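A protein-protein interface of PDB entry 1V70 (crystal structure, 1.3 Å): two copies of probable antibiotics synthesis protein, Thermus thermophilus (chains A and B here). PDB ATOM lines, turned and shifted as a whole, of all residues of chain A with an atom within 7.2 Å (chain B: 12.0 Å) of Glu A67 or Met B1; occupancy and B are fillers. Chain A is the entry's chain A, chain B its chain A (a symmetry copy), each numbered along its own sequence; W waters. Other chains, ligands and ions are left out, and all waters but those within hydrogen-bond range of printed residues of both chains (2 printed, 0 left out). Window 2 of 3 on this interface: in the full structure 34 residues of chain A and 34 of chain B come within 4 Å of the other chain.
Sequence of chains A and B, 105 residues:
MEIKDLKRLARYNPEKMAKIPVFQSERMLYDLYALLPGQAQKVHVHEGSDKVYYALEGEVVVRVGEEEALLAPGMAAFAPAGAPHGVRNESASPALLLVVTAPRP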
ATOM      1  N   VAL A  61       7.237  -1.401  22.709  1.00  0.00           N
ATOM      2  CA  VAL A  61       6.049  -0.804  22.129  1.00  0.00           C
ATOM      3  C   VAL A  61       5.458   0.050  23.240  1.00  0.00           C
ATOM      4  O   VAL A  61       5.079  -0.464  24.296  1.00  0.00           O
ATOM      5  CB  VAL A  61       5.012  -1.864  21.709  1.00  0.00           C
ATOM      6  CG1 VAL A  61       3.751  -1.175  21.205  1.00  0.00           C
ATOM      7  CG2 VAL A  61       5.589  -2.760  20.624  1.00  0.00           C
ATOM      8  N   VAL A  62       5.413   1.356  23.019  1.00  0.00           N
ATOM      9  CA  VAL A  62       4.853   2.269  24.006  1.00  0.00           C
ATOM     10  C   VAL A  62       3.437   2.644  23.591  1.00  0.00           C
ATOM     11  O   VAL A  62       3.175   2.916  22.416  1.00  0.00           O
ATOM     12  CB  VAL A  62       5.710   3.562  24.151  1.00  0.00           C
ATOM     13  CG1 VAL A  62       5.849   4.253  22.807  1.00  0.00           C
ATOM     14  CG2 VAL A  62       5.077   4.496  25.169  1.00  0.00           C
ATOM     15  N   ARG A  63       2.523   2.631  24.554  1.00  0.00           N
ATOM     16  CA  ARG A  63       1.136   2.992  24.292  1.00  0.00           C
ATOM     17  C   ARG A  63       0.804   4.236  25.096  1.00  0.00           C
ATOM     18  O   ARG A  63       1.067   4.298  26.301  1.00  0.00           O
ATOM     19  CB  ARG A  63       0.202   1.840  24.694  1.00  0.00           C
ATOM     20  CG  ARG A  63      -1.293   2.091  24.449  1.00  0.00           C
ATOM     21  CD  ARG A  63      -1.977   2.723  25.655  1.00  0.00           C
ATOM     22  NE  ARG A  63      -3.393   3.007  25.409  1.00  0.00           N
ATOM     23  CZ  ARG A  63      -4.361   2.094  25.339  1.00  0.00           C
ATOM     24  NH1 ARG A  63      -4.096   0.804  25.500  1.00  0.00           N
ATOM     25  NH2 ARG A  63      -5.609   2.479  25.099  1.00  0.00           N
ATOM     26  N   VAL A  64       0.260   5.242  24.420  1.00  0.00           N
ATOM     27  CA  VAL A  64      -0.150   6.476  25.077  1.00  0.00           C
ATOM     28  C   VAL A  64      -1.467   6.878  24.435  1.00  0.00           C
ATOM     29  O   VAL A  64      -1.520   7.161  23.238  1.00  0.00           O
ATOM     30  CB  VAL A  64       0.872   7.618  24.883  1.00  0.00           C
ATOM     31  CG1 VAL A  64       0.355   8.887  25.545  1.00  0.00           C
ATOM     32  CG2 VAL A  64       2.218   7.222  25.482  1.00  0.00           C
ATOM     33  N   GLY A  65      -2.531   6.885  25.228  1.00  0.00           N
ATOM     34  CA  GLY A  65      -3.829   7.239  24.686  1.00  0.00           C
ATOM     35  C   GLY A  65      -4.262   6.212  23.657  1.00  0.00           C
ATOM     36  O   GLY A  65      -4.194   5.011  23.909  1.00  0.00           O
ATOM     37  N   GLU A  66      -4.684   6.680  22.486  1.00  0.00           N
ATOM     38  CA  GLU A  66      -5.148   5.769  21.429  1.00  0.00           C
ATOM     39  C   GLU A  66      -4.073   5.514  20.365  1.00  0.00           C
ATOM     40  O   GLU A  66      -4.382   5.151  19.238  1.00  0.00           O
ATOM     41  CB  GLU A  66      -6.402   6.364  20.760  1.00  0.00           C
ATOM     42  CG  GLU A  66      -7.397   6.946  21.777  1.00  0.00           C
ATOM     43  CD  GLU A  66      -8.700   7.345  21.102  1.00  0.00           C
ATOM     44  OE1 GLU A  66      -8.711   7.567  19.895  1.00  0.00           O
ATOM     45  OE2 GLU A  66      -9.697   7.464  21.806  1.00  0.00           O
ATOM     46  N   GLU A  67      -2.805   5.687  20.728  1.00  0.00           N
ATOM     47  CA  GLU A  67      -1.715   5.475  19.782  1.00  0.00           C
ATOM     48  C   GLU A  67      -0.602   4.614  20.382  1.00  0.00           C
ATOM     49  O   GLU A  67      -0.381   4.620  21.593  1.00  0.00           O
ATOM     50  CB  GLU A  67      -1.140   6.832  19.362  1.00  0.00           C
ATOM     51  CG  GLU A  67      -0.156   6.804  18.197  1.00  0.00           C
ATOM     52  CD  GLU A  67       0.442   8.175  17.917  1.00  0.00           C
ATOM     53  OE1 GLU A  67       0.293   8.685  16.784  1.00  0.00           O
ATOM     54  OE2 GLU A  67       1.066   8.746  18.837  1.00  0.00           O
ATOM     55  N   GLU A  68       0.085   3.869  19.522  1.00  0.00           N
ATOM     56  CA  GLU A  68       1.214   3.042  19.934  1.00  0.00           C
ATOM     57  C   GLU A  68       2.399   3.401  19.051  1.00  0.00           C
ATOM     58  O   GLU A  68       2.229   3.847  17.910  1.00  0.00           O
ATOM     59  CB  GLU A  68       0.905   1.552  19.781  1.00  0.00           C
ATOM     60  CG  GLU A  68      -0.119   1.028  20.764  1.00  0.00           C
ATOM     61  CD  GLU A  68      -0.268  -0.475  20.684  1.00  0.00           C
ATOM     62  OE1 GLU A  68      -0.475  -0.987  19.566  1.00  0.00           O
ATOM     63  OE2 GLU A  68      -0.178  -1.140  21.735  1.00  0.00           O
ATOM     64  N   ALA A  69       3.598   3.205  19.582  1.00  0.00           N
ATOM     65  CA  ALA A  69       4.815   3.512  18.850  1.00  0.00           C
ATOM     66  C   ALA A  69       5.907   2.517  19.195  1.00  0.00           C
ATOM     67  O   ALA A  69       5.907   1.926  20.280  1.00  0.00           O
ATOM     68  CB  ALA A  69       5.284   4.922  19.189  1.00  0.00           C
ATOM     69  N   LEU A  70       6.825   2.322  18.257  1.00  0.00           N
ATOM     70  CA  LEU A  70       7.959   1.439  18.471  1.00  0.00           C
ATOM     71  C   LEU A  70       9.085   2.358  18.914  1.00  0.00           C
ATOM     72  O   LEU A  70       9.576   3.182  18.140  1.00  0.00           O
ATOM     73  CB  LEU A  70       8.335   0.715  17.174  1.00  0.00           C
ATOM     74  CG  LEU A  70       7.314  -0.298  16.653  1.00  0.00           C
ATOM     75  CD1 LEU A  70       7.876  -0.989  15.421  1.00  0.00           C
ATOM     76  CD2 LEU A  70       6.998  -1.321  17.735  1.00  0.00           C
ATOM     77  N   LEU A  71       9.469   2.227  20.175  1.00  0.00           N
ATOM     78  CA  LEU A  71      10.517   3.050  20.748  1.00  0.00           C
ATOM     79  C   LEU A  71      11.853   2.315  20.669  1.00  0.00           C
ATOM     80  O   LEU A  71      12.068   1.329  21.380  1.00  0.00           O
ATOM     81  CB  LEU A  71      10.167   3.363  22.204  1.00  0.00           C
ATOM     82  CG  LEU A  71      10.786   4.594  22.866  1.00  0.00           C
ATOM     83  CD1 LEU A  71      10.206   5.863  22.242  1.00  0.00           C
ATOM     84  CD2 LEU A  71      10.495   4.556  24.360  1.00  0.00           C
ATOM     85  N   ALA A  76      12.324   8.929  22.557  1.00  0.00           N
ATOM     86  CA  ALA A  76      11.581   9.213  23.779  1.00  0.00           C
ATOM     87  C   ALA A  76      10.116   9.481  23.455  1.00  0.00           C
ATOM     88  O   ALA A  76       9.795  10.048  22.404  1.00  0.00           O
ATOM     89  CB  ALA A  76      12.186  10.420  24.495  1.00  0.00           C
ATOM     90  N   ALA A  77       9.236   9.074  24.364  1.00  0.00           N
ATOM     91  CA  ALA A  77       7.798   9.269  24.211  1.00  0.00           C
ATOM     92  C   ALA A  77       7.246   9.891  25.491  1.00  0.00           C
ATOM     93  O   ALA A  77       7.617   9.489  26.601  1.00  0.00           O
ATOM     94  CB  ALA A  77       7.114   7.938  23.932  1.00  0.00           C
ATOM     95  N   PHE A  78       6.352  10.860  25.324  1.00  0.00           N
ATOM     96  CA  PHE A  78       5.741  11.589  26.431  1.00  0.00           C
ATOM     97  C   PHE A  78       4.310  11.118  26.725  1.00  0.00           C
ATOM     98  O   PHE A  78       3.478  11.048  25.823  1.00  0.00           O
ATOM     99  CB  PHE A  78       5.721  13.083  26.079  1.00  0.00           C
ATOM    100  CG  PHE A  78       5.247  13.974  27.191  1.00  0.00           C
ATOM    101  CD1 PHE A  78       6.101  14.328  28.230  1.00  0.00           C
ATOM    102  CD2 PHE A  78       3.947  14.471  27.197  1.00  0.00           C
ATOM    103  CE1 PHE A  78       5.669  15.167  29.260  1.00  0.00           C
ATOM    104  CE2 PHE A  78       3.505  15.309  28.222  1.00  0.00           C
ATOM    105  CZ  PHE A  78       4.368  15.656  29.254  1.00  0.00           C
ATOM    106  N   ALA A  79       4.035  10.803  27.986  1.00  0.00           N
ATOM    107  CA  ALA A  79       2.705  10.371  28.409  1.00  0.00           C
ATOM    108  C   ALA A  79       2.197  11.412  29.405  1.00  0.00           C
ATOM    109  O   ALA A  79       2.563  11.400  30.580  1.00  0.00           O
ATOM    110  CB  ALA A  79       2.779   8.999  29.069  1.00  0.00           C
ATOM    111  N   PRO A  80       1.348  12.340  28.941  1.00  0.00           N
ATOM    112  CA  PRO A  80       0.819  13.376  29.830  1.00  0.00           C
ATOM    113  C   PRO A  80      -0.156  12.851  30.875  1.00  0.00           C
ATOM    114  O   PRO A  80      -0.827  11.840  30.666  1.00  0.00           O
ATOM    115  CB  PRO A  80       0.160  14.352  28.860  1.00  0.00           C
ATOM    116  CG  PRO A  80      -0.349  13.448  27.784  1.00  0.00           C
ATOM    117  CD  PRO A  80       0.811  12.489  27.577  1.00  0.00           C
ATOM    118  N   PRO A  84      -3.950   7.217  29.434  1.00  0.00           N
ATOM    119  CA  PRO A  84      -3.615   5.829  29.759  1.00  0.00           C
ATOM    120  C   PRO A  84      -2.311   5.526  29.027  1.00  0.00           C
ATOM    121  O   PRO A  84      -2.166   5.854  27.848  1.00  0.00           O
ATOM    122  CB  PRO A  84      -4.799   5.049  29.192  1.00  0.00           C
ATOM    123  CG  PRO A  84      -5.933   6.033  29.328  1.00  0.00           C
ATOM    124  CD  PRO A  84      -5.296   7.308  28.843  1.00  0.00           C
ATOM    125  N   MET B   1       0.469  10.819  20.538  1.00  0.00           N
ATOM    126  CA  MET B   1       1.498  11.075  21.584  1.00  0.00           C
ATOM    127  C   MET B   1       2.682  11.821  20.982  1.00  0.00           C
ATOM    128  O   MET B   1       2.949  11.727  19.779  1.00  0.00           O
ATOM    129  CB  MET B   1       2.011   9.754  22.174  1.00  0.00           C
ATOM    130  CG  MET B   1       3.076   9.066  21.314  1.00  0.00           C
ATOM    131  SD  MET B   1       3.723   7.511  21.967  1.00  0.00           S
ATOM    132  CE  MET B   1       2.436   6.385  21.438  1.00  0.00           C
ATOM    133  N   GLU B   2       3.391  12.559  21.826  1.00  0.00           N
ATOM    134  CA  GLU B   2       4.577  13.246  21.386  1.00  0.00           C
ATOM    135  C   GLU B   2       5.706  12.256  21.475  1.00  0.00           C
ATOM    136  O   GLU B   2       5.877  11.578  22.475  1.00  0.00           O
ATOM    137  CB  GLU B   2       4.844  14.457  22.300  1.00  0.00           C
ATOM    138  CG  GLU B   2       3.822  15.595  22.122  1.00  0.00           C
ATOM    139  CD  GLU B   2       4.152  16.778  23.025  1.00  0.00           C
ATOM    140  OE1 GLU B   2       5.279  17.238  23.011  1.00  0.00           O
ATOM    141  OE2 GLU B   2       3.246  17.268  23.692  1.00  0.00           O
ATOM    142  N   ILE B   3       6.461  12.133  20.394  1.00  0.00           N
ATOM    143  CA  ILE B   3       7.567  11.190  20.340  1.00  0.00           C
ATOM    144  C   ILE B   3       8.667  11.807  19.490  1.00  0.00           C
ATOM    145  O   ILE B   3       8.402  12.412  18.448  1.00  0.00           O
ATOM    146  CB  ILE B   3       7.091   9.831  19.765  1.00  0.00           C
ATOM    147  CG1 ILE B   3       8.243   8.825  19.761  1.00  0.00           C
ATOM    148  CG2 ILE B   3       6.507  10.030  18.376  1.00  0.00           C
ATOM    149  CD1 ILE B   3       7.789   7.392  19.550  1.00  0.00           C
ATOM    150  N   LYS B   4       9.905  11.678  19.949  1.00  0.00           N
ATOM    151  CA  LYS B   4      11.038  12.268  19.250  1.00  0.00           C
ATOM    152  C   LYS B   4      12.252  11.362  19.244  1.00  0.00           C
ATOM    153  O   LYS B   4      12.452  10.571  20.165  1.00  0.00           O
ATOM    154  CB  LYS B   4      11.441  13.585  19.927  1.00  0.00           C
ATOM    155  CG  LYS B   4      10.389  14.687  19.906  1.00  0.00           C
ATOM    156  CD  LYS B   4      10.282  15.313  18.526  1.00  0.00           C
ATOM    157  CE  LYS B   4       9.243  16.422  18.503  1.00  0.00           C
ATOM    158  NZ  LYS B   4       9.206  17.096  17.178  1.00  0.00           N
ATOM    159  N   ASP B   5      13.061  11.485  18.198  1.00  0.00           N
ATOM    160  CA  ASP B   5      14.304  10.733  18.099  1.00  0.00           C
ATOM    161  C   ASP B   5      15.328  11.770  18.556  1.00  0.00           C
ATOM    162  O   ASP B   5      15.658  12.694  17.806  1.00  0.00           O
ATOM    163  CB  ASP B   5      14.587  10.322  16.652  1.00  0.00           C
ATOM    164  CG  ASP B   5      15.869   9.518  16.517  1.00  0.00           C
ATOM    165  OD1 ASP B   5      16.706   9.578  17.444  1.00  0.00           O
ATOM    166  OD2 ASP B   5      16.049   8.836  15.487  1.00  0.00           O
ATOM    167  N   LEU B   6      15.808  11.638  19.788  1.00  0.00           N
ATOM    168  CA  LEU B   6      16.766  12.594  20.332  1.00  0.00           C
ATOM    169  C   LEU B   6      18.028  12.731  19.494  1.00  0.00           C
ATOM    170  O   LEU B   6      18.656  13.793  19.479  1.00  0.00           O
ATOM    171  CB  LEU B   6      17.127  12.223  21.773  1.00  0.00           C
ATOM    172  CG  LEU B   6      16.114  12.628  22.852  1.00  0.00           C
ATOM    173  CD1 LEU B   6      14.731  12.087  22.529  1.00  0.00           C
ATOM    174  CD2 LEU B   6      16.592  12.119  24.203  1.00  0.00           C
ATOM    175  N   ARG B   8      18.178  12.858  16.362  1.00  0.00           N
ATOM    176  CA  ARG B   8      17.882  13.817  15.293  1.00  0.00           C
ATOM    177  C   ARG B   8      17.876  15.257  15.795  1.00  0.00           C
ATOM    178  O   ARG B   8      18.286  16.165  15.084  1.00  0.00           O
ATOM    179  CB  ARG B   8      16.525  13.483  14.679  1.00  0.00           C
ATOM    180  CG  ARG B   8      16.160  14.436  13.534  1.00  0.00           C
ATOM    181  CD  ARG B   8      14.630  14.591  13.387  1.00  0.00           C
ATOM    182  NE  ARG B   8      14.327  15.932  12.877  1.00  0.00           N
ATOM    183  CZ  ARG B   8      13.262  16.621  13.363  1.00  0.00           C
ATOM    184  NH1 ARG B   8      12.472  16.107  14.307  1.00  0.00           N
ATOM    185  NH2 ARG B   8      13.009  17.833  12.878  1.00  0.00           N
ATOM    186  N   VAL B  22      12.821  19.104  24.328  1.00  0.00           N
ATOM    187  CA  VAL B  22      12.276  17.893  23.729  1.00  0.00           C
ATOM    188  C   VAL B  22      10.781  17.880  24.049  1.00  0.00           C
ATOM    189  O   VAL B  22       9.944  17.884  23.146  1.00  0.00           O
ATOM    190  CB  VAL B  22      12.959  16.628  24.301  1.00  0.00           C
ATOM    191  CG1 VAL B  22      12.386  15.382  23.635  1.00  0.00           C
ATOM    192  CG2 VAL B  22      14.465  16.700  24.069  1.00  0.00           C
ATOM    193  N   PHE B  23      10.462  17.875  25.340  1.00  0.00           N
ATOM    194  CA  PHE B  23       9.084  17.904  25.827  1.00  0.00           C
ATOM    195  C   PHE B  23       9.033  18.913  26.966  1.00  0.00           C
ATOM    196  O   PHE B  23      10.038  19.157  27.641  1.00  0.00           O
ATOM    197  CB  PHE B  23       8.644  16.553  26.393  1.00  0.00           C
ATOM    198  CG  PHE B  23       8.817  15.398  25.451  1.00  0.00           C
ATOM    199  CD1 PHE B  23       8.185  15.377  24.211  1.00  0.00           C
ATOM    200  CD2 PHE B  23       9.601  14.311  25.825  1.00  0.00           C
ATOM    201  CE1 PHE B  23       8.332  14.281  23.359  1.00  0.00           C
ATOM    202  CE2 PHE B  23       9.754  13.220  24.987  1.00  0.00           C
ATOM    203  CZ  PHE B  23       9.119  13.201  23.752  1.00  0.00           C
ATOM    204  N   GLN B  24       7.859  19.486  27.200  1.00  0.00           N
ATOM    205  CA  GLN B  24       7.717  20.452  28.287  1.00  0.00           C
ATOM    206  C   GLN B  24       6.283  20.543  28.775  1.00  0.00           C
ATOM    207  O   GLN B  24       5.333  20.417  28.015  1.00  0.00           O
ATOM    208  CB  GLN B  24       8.229  21.828  27.810  1.00  0.00           C
ATOM    209  CG  GLN B  24       7.351  22.510  26.732  1.00  0.00           C
ATOM    210  CD  GLN B  24       7.506  21.799  25.397  1.00  0.00           C
ATOM    211  OE1 GLN B  24       6.731  20.932  25.025  1.00  0.00           O
ATOM    212  NE2 GLN B  24       8.523  22.254  24.632  1.00  0.00           N
HETATM  213  O   HOH W   1       2.223  12.957  24.315  1.00  0.00           O
HETATM  214  O   HOH W   2      -1.525   9.721  22.169  1.00  0.00           O
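Glu A67 touches just one residue of chain B: Met B1 (2.7 Å). Of the printed residues of chain A, Met B1 touches Val A62 (3.7 Å), Val A64 (3.6 Å), Glu A67 (2.7 Å), Glu A68 (3.8 Å), Ala A69 (3.9 Å) and Ala A77 (3.9 Å). Val A64 touches just one residue of chain B: Met B1 (3.6 Å). Gly A65 touches none of the printed residues of chain B. Glu A68 touches just one residue of chain B: Met B1. Of chain B, only Met B1 and Ile B3 come within 4 Å of Ala A69. Of chain B, only Met B1 and Glu B2 come within 4 Å of Ala A77. Printed residues of chain B within 4 Å of Leu A71: Ile B3 (3.9 Å). Of the printed residues of chain A, Lys B4 touches Ala A76. Of the printed residues of chain A, Phe B23 touches Ala A76 (3.5 Å) and Phe A78 (3.8 Å). Printed residues of chain B within 4 Å of Val A62: Met B1 (3.7 Å). Of the printed residues of chain A, Leu B6 touches Ala A76. The nearest residue of chain B that does not touch Glu A67 is Glu B2 (5.4 Å). The nearest printed residue of chain A that does not touch Ile B3 is Ala A77 (4.3 Å).
The backbone NH of Met B1 is in hydrogen-bond range of the side-chain carboxylate of Glu A67 (2.7 Å). N of Ala A76 lies within hydrogen-bond range of O of Lys B4 (2.9 Å). The backbone NH (N) of Phe A78 is in hydrogen-bond range of the backbone carbonyl oxygen (O) of Glu B2, 3.0 Å away.
Water W1 bridges the backbone carbonyl oxygen (O) of Phe A78 and the backbone NH (N) of Glu B2. Water W2 lies within hydrogen-bond range of O of Val A64 (2.8 Å) and N of Met B1 (2.8 Å).
No position is printed for both chains. Of the 15 pairs that touch across the chains among the printed residues, none has its exchanged pair printed and touching as well.
Hydrophobic or aromatic side chains of chain B that line the printed part of chain A: Met B1, Ile B3, Leu B6 and Phe B23. Hydrophobic or aromatic side chains of chain A within 4 Å of the printed part of chain B: Val A62, Val A64, Ala A69, Leu A71, Ala A76, Ala A77 and Phe A78. Along chain A the printed residues that touch a printed residue of chain B span positions 62 to 78. Among the printed residues, no Asp or Glu carboxylate lies within 4 Å of a Lys or Arg side-chain nitrogen of the other chain.
O of Ala A69 sits at hydrogen-bond distance from N of Val A62.
Among the printed residues, pairs that only touch across the chains: Val A62 with Met B1 (3.7 Å), Val A64 with Met B1 (3.6 Å), Glu A68 with Met B1 (3.8 Å), Ala A69 with Met B1 (3.9 Å), Ala A69 with Ile B3 (3.5 Å), Leu A71 with Ile B3 (3.9 Å), Ala A76 with Ile B3 (3.2 Å), Ala A76 with Leu B6 (3.6 Å), Ala A76 with Phe B23 (3.5 Å), Ala A77 with Met B1 (3.9 Å), Ala A77 with Glu B2 (3.5 Å) and Phe A78 with Phe B23 (3.8 Å).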
